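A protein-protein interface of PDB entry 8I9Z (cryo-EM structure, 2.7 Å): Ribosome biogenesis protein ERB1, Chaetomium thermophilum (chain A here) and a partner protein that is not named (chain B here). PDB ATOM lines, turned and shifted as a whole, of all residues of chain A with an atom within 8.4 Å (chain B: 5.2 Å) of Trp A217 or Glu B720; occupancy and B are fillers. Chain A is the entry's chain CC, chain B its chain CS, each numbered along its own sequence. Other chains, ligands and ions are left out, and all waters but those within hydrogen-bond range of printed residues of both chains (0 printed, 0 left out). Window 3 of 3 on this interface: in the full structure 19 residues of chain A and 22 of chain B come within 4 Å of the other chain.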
ATOM      1  N   ASP A 209      -2.803 -25.891  10.277  1.00  0.00           N
ATOM      2  CA  ASP A 209      -4.177 -25.623   9.864  1.00  0.00           C
ATOM      3  C   ASP A 209      -4.219 -24.853   8.553  1.00  0.00           C
ATOM      4  O   ASP A 209      -5.216 -24.908   7.823  1.00  0.00           O
ATOM      5  CB  ASP A 209      -4.931 -24.856  10.950  1.00  0.00           C
ATOM      6  CG  ASP A 209      -4.607 -25.344  12.341  1.00  0.00           C
ATOM      7  OD1 ASP A 209      -4.344 -26.554  12.500  1.00  0.00           O
ATOM      8  OD2 ASP A 209      -4.614 -24.520  13.279  1.00  0.00           O
ATOM      9  N   SER A 210      -3.152 -24.119   8.244  1.00  0.00           N
ATOM     10  CA  SER A 210      -3.079 -23.426   6.966  1.00  0.00           C
ATOM     11  C   SER A 210      -2.920 -24.409   5.815  1.00  0.00           C
ATOM     12  O   SER A 210      -3.424 -24.171   4.711  1.00  0.00           O
ATOM     13  CB  SER A 210      -1.928 -22.425   6.983  1.00  0.00           C
ATOM     14  OG  SER A 210      -1.788 -21.835   8.263  1.00  0.00           O
ATOM     15  N   ILE A 211      -2.218 -25.517   6.049  1.00  0.00           N
ATOM     16  CA  ILE A 211      -1.987 -26.494   4.989  1.00  0.00           C
ATOM     17  C   ILE A 211      -3.110 -27.521   4.959  1.00  0.00           C
ATOM     18  O   ILE A 211      -3.839 -27.644   3.969  1.00  0.00           O
ATOM     19  CB  ILE A 211      -0.618 -27.164   5.174  1.00  0.00           C
ATOM     20  CG1 ILE A 211       0.479 -26.109   5.067  1.00  0.00           C
ATOM     21  CG2 ILE A 211      -0.427 -28.268   4.145  1.00  0.00           C
ATOM     22  CD1 ILE A 211       1.854 -26.669   5.019  1.00  0.00           C
ATOM     23  N   GLU A 212      -3.265 -28.270   6.040  1.00  0.00           N
ATOM     24  CA  GLU A 212      -4.345 -29.237   6.188  1.00  0.00           C
ATOM     25  C   GLU A 212      -5.420 -28.569   7.038  1.00  0.00           C
ATOM     26  O   GLU A 212      -5.352 -28.563   8.267  1.00  0.00           O
ATOM     27  CB  GLU A 212      -3.844 -30.533   6.809  1.00  0.00           C
ATOM     28  CG  GLU A 212      -2.677 -31.152   6.061  1.00  0.00           C
ATOM     29  CD  GLU A 212      -2.151 -32.405   6.732  1.00  0.00           C
ATOM     30  OE1 GLU A 212      -2.279 -32.518   7.968  1.00  0.00           O
ATOM     31  OE2 GLU A 212      -1.614 -33.279   6.018  1.00  0.00           O
ATOM     32  N   VAL A 213      -6.408 -27.992   6.360  1.00  0.00           N
ATOM     33  CA  VAL A 213      -7.494 -27.240   6.981  1.00  0.00           C
ATOM     34  C   VAL A 213      -8.340 -28.203   7.805  1.00  0.00           C
ATOM     35  O   VAL A 213      -8.575 -29.337   7.364  1.00  0.00           O
ATOM     36  CB  VAL A 213      -8.330 -26.517   5.914  1.00  0.00           C
ATOM     37  CG1 VAL A 213      -9.082 -25.351   6.506  1.00  0.00           C
ATOM     38  CG2 VAL A 213      -7.443 -26.046   4.777  1.00  0.00           C
ATOM     39  N   PRO A 214      -8.790 -27.819   8.999  1.00  0.00           N
ATOM     40  CA  PRO A 214      -9.648 -28.709   9.788  1.00  0.00           C
ATOM     41  C   PRO A 214     -10.994 -28.953   9.121  1.00  0.00           C
ATOM     42  O   PRO A 214     -11.433 -28.210   8.243  1.00  0.00           O
ATOM     43  CB  PRO A 214      -9.812 -27.962  11.114  1.00  0.00           C
ATOM     44  CG  PRO A 214      -8.636 -27.075  11.189  1.00  0.00           C
ATOM     45  CD  PRO A 214      -8.342 -26.661   9.788  1.00  0.00           C
ATOM     46  N   GLU A 215     -11.633 -30.049   9.538  1.00  0.00           N
ATOM     47  CA  GLU A 215     -12.879 -30.474   8.908  1.00  0.00           C
ATOM     48  C   GLU A 215     -14.010 -29.491   9.178  1.00  0.00           C
ATOM     49  O   GLU A 215     -14.772 -29.146   8.269  1.00  0.00           O
ATOM     50  CB  GLU A 215     -13.255 -31.873   9.400  1.00  0.00           C
ATOM     51  CG  GLU A 215     -14.534 -32.427   8.797  1.00  0.00           C
ATOM     52  CD  GLU A 215     -14.811 -33.853   9.229  1.00  0.00           C
ATOM     53  OE1 GLU A 215     -13.842 -34.626   9.385  1.00  0.00           O
ATOM     54  OE2 GLU A 215     -15.995 -34.201   9.414  1.00  0.00           O
ATOM     55  N   GLY A 216     -14.127 -29.017  10.415  1.00  0.00           N
ATOM     56  CA  GLY A 216     -15.205 -28.120  10.771  1.00  0.00           C
ATOM     57  C   GLY A 216     -14.814 -26.663  10.663  1.00  0.00           C
ATOM     58  O   GLY A 216     -15.416 -25.802  11.308  1.00  0.00           O
ATOM     59  N   TRP A 217     -13.794 -26.390   9.856  1.00  0.00           N
ATOM     60  CA  TRP A 217     -13.244 -25.049   9.737  1.00  0.00           C
ATOM     61  C   TRP A 217     -14.247 -24.100   9.097  1.00  0.00           C
ATOM     62  O   TRP A 217     -14.941 -24.452   8.141  1.00  0.00           O
ATOM     63  CB  TRP A 217     -11.963 -25.092   8.919  1.00  0.00           C
ATOM     64  CG  TRP A 217     -11.314 -23.785   8.712  1.00  0.00           C
ATOM     65  CD1 TRP A 217     -10.450 -23.154   9.551  1.00  0.00           C
ATOM     66  CD2 TRP A 217     -11.455 -22.943   7.573  1.00  0.00           C
ATOM     67  NE1 TRP A 217     -10.045 -21.965   9.005  1.00  0.00           N
ATOM     68  CE2 TRP A 217     -10.653 -21.813   7.789  1.00  0.00           C
ATOM     69  CE3 TRP A 217     -12.187 -23.036   6.387  1.00  0.00           C
ATOM     70  CZ2 TRP A 217     -10.562 -20.785   6.866  1.00  0.00           C
ATOM     71  CZ3 TRP A 217     -12.095 -22.012   5.473  1.00  0.00           C
ATOM     72  CH2 TRP A 217     -11.292 -20.903   5.719  1.00  0.00           C
ATOM     73  N   THR A 218     -14.315 -22.891   9.635  1.00  0.00           N
ATOM     74  CA  THR A 218     -15.299 -21.904   9.222  1.00  0.00           C
ATOM     75  C   THR A 218     -14.690 -20.610   8.712  1.00  0.00           C
ATOM     76  O   THR A 218     -15.217 -20.033   7.762  1.00  0.00           O
ATOM     77  CB  THR A 218     -16.242 -21.584  10.391  1.00  0.00           C
ATOM     78  OG1 THR A 218     -16.537 -22.786  11.111  1.00  0.00           O
ATOM     79  CG2 THR A 218     -17.540 -20.982   9.893  1.00  0.00           C
ATOM     80  N   GLY A 219     -13.586 -20.156   9.291  1.00  0.00           N
ATOM     81  CA  GLY A 219     -13.041 -18.856   8.976  1.00  0.00           C
ATOM     82  C   GLY A 219     -13.554 -17.737   9.848  1.00  0.00           C
ATOM     83  O   GLY A 219     -13.329 -16.567   9.522  1.00  0.00           O
ATOM     84  N   LEU A 220     -14.235 -18.058  10.941  1.00  0.00           N
ATOM     85  CA  LEU A 220     -14.818 -17.087  11.849  1.00  0.00           C
ATOM     86  C   LEU A 220     -14.049 -17.067  13.162  1.00  0.00           C
ATOM     87  O   LEU A 220     -13.218 -17.935  13.436  1.00  0.00           O
ATOM     88  CB  LEU A 220     -16.289 -17.412  12.127  1.00  0.00           C
ATOM     89  CG  LEU A 220     -17.299 -17.272  10.994  1.00  0.00           C
ATOM     90  CD1 LEU A 220     -18.710 -17.422  11.536  1.00  0.00           C
ATOM     91  CD2 LEU A 220     -17.140 -15.948  10.274  1.00  0.00           C
ATOM     92  N   PRO A 228     -10.138 -19.440  16.743  1.00  0.00           N
ATOM     93  CA  PRO A 228     -11.025 -19.700  15.603  1.00  0.00           C
ATOM     94  C   PRO A 228     -12.130 -20.686  15.945  1.00  0.00           C
ATOM     95  O   PRO A 228     -11.921 -21.668  16.658  1.00  0.00           O
ATOM     96  CB  PRO A 228     -10.077 -20.262  14.537  1.00  0.00           C
ATOM     97  CG  PRO A 228      -8.857 -20.683  15.279  1.00  0.00           C
ATOM     98  CD  PRO A 228      -8.733 -19.710  16.399  1.00  0.00           C
ATOM     99  N   LEU A 229     -13.314 -20.407  15.417  1.00  0.00           N
ATOM    100  CA  LEU A 229     -14.513 -21.162  15.742  1.00  0.00           C
ATOM    101  C   LEU A 229     -14.746 -22.267  14.724  1.00  0.00           C
ATOM    102  O   LEU A 229     -14.772 -22.020  13.515  1.00  0.00           O
ATOM    103  CB  LEU A 229     -15.701 -20.210  15.805  1.00  0.00           C
ATOM    104  CG  LEU A 229     -17.100 -20.781  15.688  1.00  0.00           C
ATOM    105  CD1 LEU A 229     -17.969 -20.326  16.830  1.00  0.00           C
ATOM    106  CD2 LEU A 229     -17.635 -20.246  14.395  1.00  0.00           C
ATOM    107  N   ASN A 230     -14.925 -23.488  15.221  1.00  0.00           N
ATOM    108  CA  ASN A 230     -14.950 -24.686  14.398  1.00  0.00           C
ATOM    109  C   ASN A 230     -16.263 -25.425  14.596  1.00  0.00           C
ATOM    110  O   ASN A 230     -16.770 -25.509  15.718  1.00  0.00           O
ATOM    111  CB  ASN A 230     -13.777 -25.603  14.741  1.00  0.00           C
ATOM    112  CG  ASN A 230     -12.529 -25.271  13.951  1.00  0.00           C
ATOM    113  OD1 ASN A 230     -12.453 -24.233  13.299  1.00  0.00           O
ATOM    114  ND2 ASN A 230     -11.541 -26.155  14.007  1.00  0.00           N
ATOM    115  N   LEU A 231     -16.808 -25.954  13.505  1.00  0.00           N
ATOM    116  CA  LEU A 231     -18.034 -26.733  13.572  1.00  0.00           C
ATOM    117  C   LEU A 231     -17.764 -28.109  14.160  1.00  0.00           C
ATOM    118  O   LEU A 231     -16.729 -28.724  13.895  1.00  0.00           O
ATOM    119  CB  LEU A 231     -18.644 -26.873  12.182  1.00  0.00           C
ATOM    120  CG  LEU A 231     -19.043 -25.584  11.470  1.00  0.00           C
ATOM    121  CD1 LEU A 231     -18.941 -25.775   9.970  1.00  0.00           C
ATOM    122  CD2 LEU A 231     -20.450 -25.191  11.854  1.00  0.00           C
ATOM    123  N   SER A 232     -18.705 -28.594  14.960  1.00  0.00           N
ATOM    124  CA  SER A 232     -18.585 -29.912  15.553  1.00  0.00           C
ATOM    125  C   SER A 232     -19.005 -30.985  14.556  1.00  0.00           C
ATOM    126  O   SER A 232     -19.536 -30.701  13.479  1.00  0.00           O
ATOM    127  CB  SER A 232     -19.417 -30.000  16.830  1.00  0.00           C
ATOM    128  OG  SER A 232     -20.782 -29.735  16.572  1.00  0.00           O
ATOM    129  N   LEU A 236     -21.670 -30.777  11.454  1.00  0.00           N
ATOM    130  CA  LEU A 236     -21.333 -31.063  10.062  1.00  0.00           C
ATOM    131  C   LEU A 236     -22.287 -32.084   9.457  1.00  0.00           C
ATOM    132  O   LEU A 236     -22.552 -32.057   8.250  1.00  0.00           O
ATOM    133  CB  LEU A 236     -19.892 -31.555   9.954  1.00  0.00           C
ATOM    134  CG  LEU A 236     -18.788 -30.509  10.080  1.00  0.00           C
ATOM    135  CD1 LEU A 236     -17.519 -31.145  10.608  1.00  0.00           C
ATOM    136  CD2 LEU A 236     -18.537 -29.851   8.740  1.00  0.00           C
ATOM    137  N   ILE A 239     -25.476 -30.160   8.387  1.00  0.00           N
ATOM    138  CA  ILE A 239     -25.293 -29.383   7.164  1.00  0.00           C
ATOM    139  C   ILE A 239     -25.396 -30.286   5.945  1.00  0.00           C
ATOM    140  O   ILE A 239     -25.995 -29.917   4.926  1.00  0.00           O
ATOM    141  CB  ILE A 239     -23.941 -28.652   7.216  1.00  0.00           C
ATOM    142  CG1 ILE A 239     -23.908 -27.717   8.423  1.00  0.00           C
ATOM    143  CG2 ILE A 239     -23.687 -27.886   5.922  1.00  0.00           C
ATOM    144  CD1 ILE A 239     -22.818 -26.703   8.386  1.00  0.00           C
ATOM    145  N   MET B 660     -21.063 -23.343   2.819  1.00  0.00           N
ATOM    146  CA  MET B 660     -20.364 -22.423   3.711  1.00  0.00           C
ATOM    147  C   MET B 660     -21.328 -21.406   4.302  1.00  0.00           C
ATOM    148  O   MET B 660     -21.212 -21.038   5.477  1.00  0.00           O
ATOM    149  CB  MET B 660     -19.245 -21.715   2.947  1.00  0.00           C
ATOM    150  CG  MET B 660     -17.942 -21.438   3.704  1.00  0.00           C
ATOM    151  SD  MET B 660     -17.318 -22.724   4.801  1.00  0.00           S
ATOM    152  CE  MET B 660     -17.819 -22.087   6.384  1.00  0.00           C
ATOM    153  N   GLN B 716     -15.599 -15.967   0.435  1.00  0.00           N
ATOM    154  CA  GLN B 716     -14.198 -15.685   0.726  1.00  0.00           C
ATOM    155  C   GLN B 716     -13.543 -16.849   1.455  1.00  0.00           C
ATOM    156  O   GLN B 716     -12.364 -17.146   1.235  1.00  0.00           O
ATOM    157  CB  GLN B 716     -14.087 -14.400   1.543  1.00  0.00           C
ATOM    158  CG  GLN B 716     -12.671 -13.921   1.764  1.00  0.00           C
ATOM    159  CD  GLN B 716     -12.617 -12.487   2.228  1.00  0.00           C
ATOM    160  OE1 GLN B 716     -13.079 -11.581   1.535  1.00  0.00           O
ATOM    161  NE2 GLN B 716     -12.061 -12.270   3.413  1.00  0.00           N
ATOM    162  N   ALA B 717     -14.297 -17.525   2.320  1.00  0.00           N
ATOM    163  CA  ALA B 717     -13.750 -18.663   3.045  1.00  0.00           C
ATOM    164  C   ALA B 717     -13.481 -19.831   2.110  1.00  0.00           C
ATOM    165  O   ALA B 717     -12.540 -20.601   2.325  1.00  0.00           O
ATOM    166  CB  ALA B 717     -14.704 -19.076   4.162  1.00  0.00           C
ATOM    167  N   ILE B 718     -14.298 -19.979   1.070  1.00  0.00           N
ATOM    168  CA  ILE B 718     -14.166 -21.111   0.161  1.00  0.00           C
ATOM    169  C   ILE B 718     -12.924 -20.973  -0.715  1.00  0.00           C
ATOM    170  O   ILE B 718     -12.183 -21.944  -0.909  1.00  0.00           O
ATOM    171  CB  ILE B 718     -15.457 -21.264  -0.662  1.00  0.00           C
ATOM    172  CG1 ILE B 718     -16.556 -21.830   0.232  1.00  0.00           C
ATOM    173  CG2 ILE B 718     -15.252 -22.144  -1.872  1.00  0.00           C
ATOM    174  CD1 ILE B 718     -16.182 -23.138   0.899  1.00  0.00           C
ATOM    175  N   LYS B 719     -12.669 -19.774  -1.250  1.00  0.00           N
ATOM    176  CA  LYS B 719     -11.485 -19.589  -2.085  1.00  0.00           C
ATOM    177  C   LYS B 719     -10.205 -19.718  -1.273  1.00  0.00           C
ATOM    178  O   LYS B 719      -9.197 -20.234  -1.768  1.00  0.00           O
ATOM    179  CB  LYS B 719     -11.518 -18.238  -2.796  1.00  0.00           C
ATOM    180  CG  LYS B 719     -12.523 -18.153  -3.928  1.00  0.00           C
ATOM    181  CD  LYS B 719     -12.696 -16.763  -4.583  1.00  0.00           C
ATOM    182  CE  LYS B 719     -12.483 -15.487  -3.746  1.00  0.00           C
ATOM    183  NZ  LYS B 719     -12.930 -15.441  -2.329  1.00  0.00           N
ATOM    184  N   GLU B 720     -10.218 -19.249  -0.027  1.00  0.00           N
ATOM    185  CA  GLU B 720      -9.016 -19.340   0.788  1.00  0.00           C
ATOM    186  C   GLU B 720      -8.848 -20.751   1.348  1.00  0.00           C
ATOM    187  O   GLU B 720      -7.730 -21.175   1.664  1.00  0.00           O
ATOM    188  CB  GLU B 720      -9.052 -18.244   1.863  1.00  0.00           C
ATOM    189  CG  GLU B 720      -8.323 -18.478   3.174  1.00  0.00           C
ATOM    190  CD  GLU B 720      -8.963 -17.726   4.324  1.00  0.00           C
ATOM    191  OE1 GLU B 720      -9.515 -18.367   5.233  1.00  0.00           O
ATOM    192  OE2 GLU B 720      -8.916 -16.478   4.312  1.00  0.00           O
ATOM    193  N   LYS B 721      -9.936 -21.519   1.407  1.00  0.00           N
ATOM    194  CA  LYS B 721      -9.824 -22.941   1.723  1.00  0.00           C
ATOM    195  C   LYS B 721      -9.292 -23.736   0.537  1.00  0.00           C
ATOM    196  O   LYS B 721      -8.475 -24.647   0.710  1.00  0.00           O
ATOM    197  CB  LYS B 721     -11.179 -23.491   2.162  1.00  0.00           C
ATOM    198  CG  LYS B 721     -11.174 -24.938   2.595  1.00  0.00           C
ATOM    199  CD  LYS B 721     -12.585 -25.489   2.638  1.00  0.00           C
ATOM    200  CE  LYS B 721     -12.641 -26.842   3.315  1.00  0.00           C
ATOM    201  NZ  LYS B 721     -12.744 -26.725   4.792  1.00  0.00           N
ATOM    202  N   LEU B 722      -9.737 -23.405  -0.671  1.00  0.00           N
ATOM    203  CA  LEU B 722      -9.387 -24.153  -1.869  1.00  0.00           C
ATOM    204  C   LEU B 722      -8.183 -23.582  -2.600  1.00  0.00           C
ATOM    205  O   LEU B 722      -7.881 -24.030  -3.710  1.00  0.00           O
ATOM    206  CB  LEU B 722     -10.582 -24.211  -2.821  1.00  0.00           C
ATOM    207  CG  LEU B 722     -11.783 -25.019  -2.338  1.00  0.00           C
ATOM    208  CD1 LEU B 722     -12.842 -25.070  -3.419  1.00  0.00           C
ATOM    209  CD2 LEU B 722     -11.360 -26.415  -1.938  1.00  0.00           C
ATOM    210  N   ARG B 723      -7.503 -22.598  -2.021  1.00  0.00           N
ATOM    211  CA  ARG B 723      -6.280 -22.088  -2.621  1.00  0.00           C
ATOM    212  C   ARG B 723      -5.168 -23.121  -2.521  1.00  0.00           C
ATOM    213  O   ARG B 723      -5.010 -23.794  -1.499  1.00  0.00           O
ATOM    214  CB  ARG B 723      -5.859 -20.792  -1.934  1.00  0.00           C
ATOM    215  CG  ARG B 723      -4.914 -19.943  -2.747  1.00  0.00           C
ATOM    216  CD  ARG B 723      -4.653 -18.621  -2.063  1.00  0.00           C
ATOM    217  NE  ARG B 723      -3.785 -18.775  -0.905  1.00  0.00           N
ATOM    218  CZ  ARG B 723      -3.081 -17.790  -0.366  1.00  0.00           C
ATOM    219  NH1 ARG B 723      -3.104 -16.568  -0.869  1.00  0.00           N
ATOM    220  NH2 ARG B 723      -2.335 -18.038   0.706  1.00  0.00           N
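The backbone carbonyl oxygen (O) of Gly A216 is in hydrogen-bond range of the side-chain hydroxyl (OG1) of Thr A218 (3.2 Å).
The backbone carbonyl oxygen (O) of Leu A229 lies within hydrogen-bond range of the side-chain hydroxyl (OG1) of Thr A218, 3.1 Å away.
O of Pro A214 touches NZ of Lys B721, 3.98 Å away.
Trp A217 touches Ala B717.
Trp A217 touches Glu B720 (CZ2 to OE1, 3.1 Å).
CZ3 of Trp A217 touches CB of Lys B721, at 3.7 Å.
Thr A218 touches Met B660 (O to CE, 3.6 Å).
Thr A218 touches Ala B717 (O to CB, 3.8 Å).
Of the printed residues of chain B, Pro A214 touches Lys B721 (3.98 Å).
Glu A215 touches none of the printed residues of chain B.
Of chain B, only Ala B717 (3.5 Å), Glu B720 (3.1 Å) and Lys B721 (3.7 Å) come within 4 Å of Trp A217.
Printed residues of chain B within 4 Å of Thr A218: Met B660 (3.6 Å) and Ala B717 (3.8 Å).
Printed residues of chain A within 4 Å of Ala B717: Trp A217 and Thr A218.
Printed residues of chain A within 4 Å of Lys B721: Pro A214 (3.98 Å) and Trp A217 (3.7 Å).
Leu B722 touches none of the printed residues of chain A.
The nearest residue of chain B that does not touch Trp A217 is Met B660 (4.1 Å).
The nearest residue of chain A that does not touch Glu B720 is Gly A219 (5.2 Å).
The nearest printed residue of chain A that does not touch Ala B717 is Gly A219 (5.1 Å).
Of the 9 printed residues of chain B, 4 touch a printed residue of chain A.
Printed residues of chain B that touch a printed residue of chain A: Met B660, Ala B717, Glu B720 and Lys B721.
Of the 19 printed residues of chain A, 3 touch a printed residue of chain B.
Hydrophobic or aromatic side chains of chain A that line the printed part of chain B: Trp A217.
Among the printed residues, 6 pairs touch across the chains.
Among the printed residues, no Asp or Glu carboxylate lies within 4 Å of a Lys or Arg side-chain nitrogen of the other chain.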
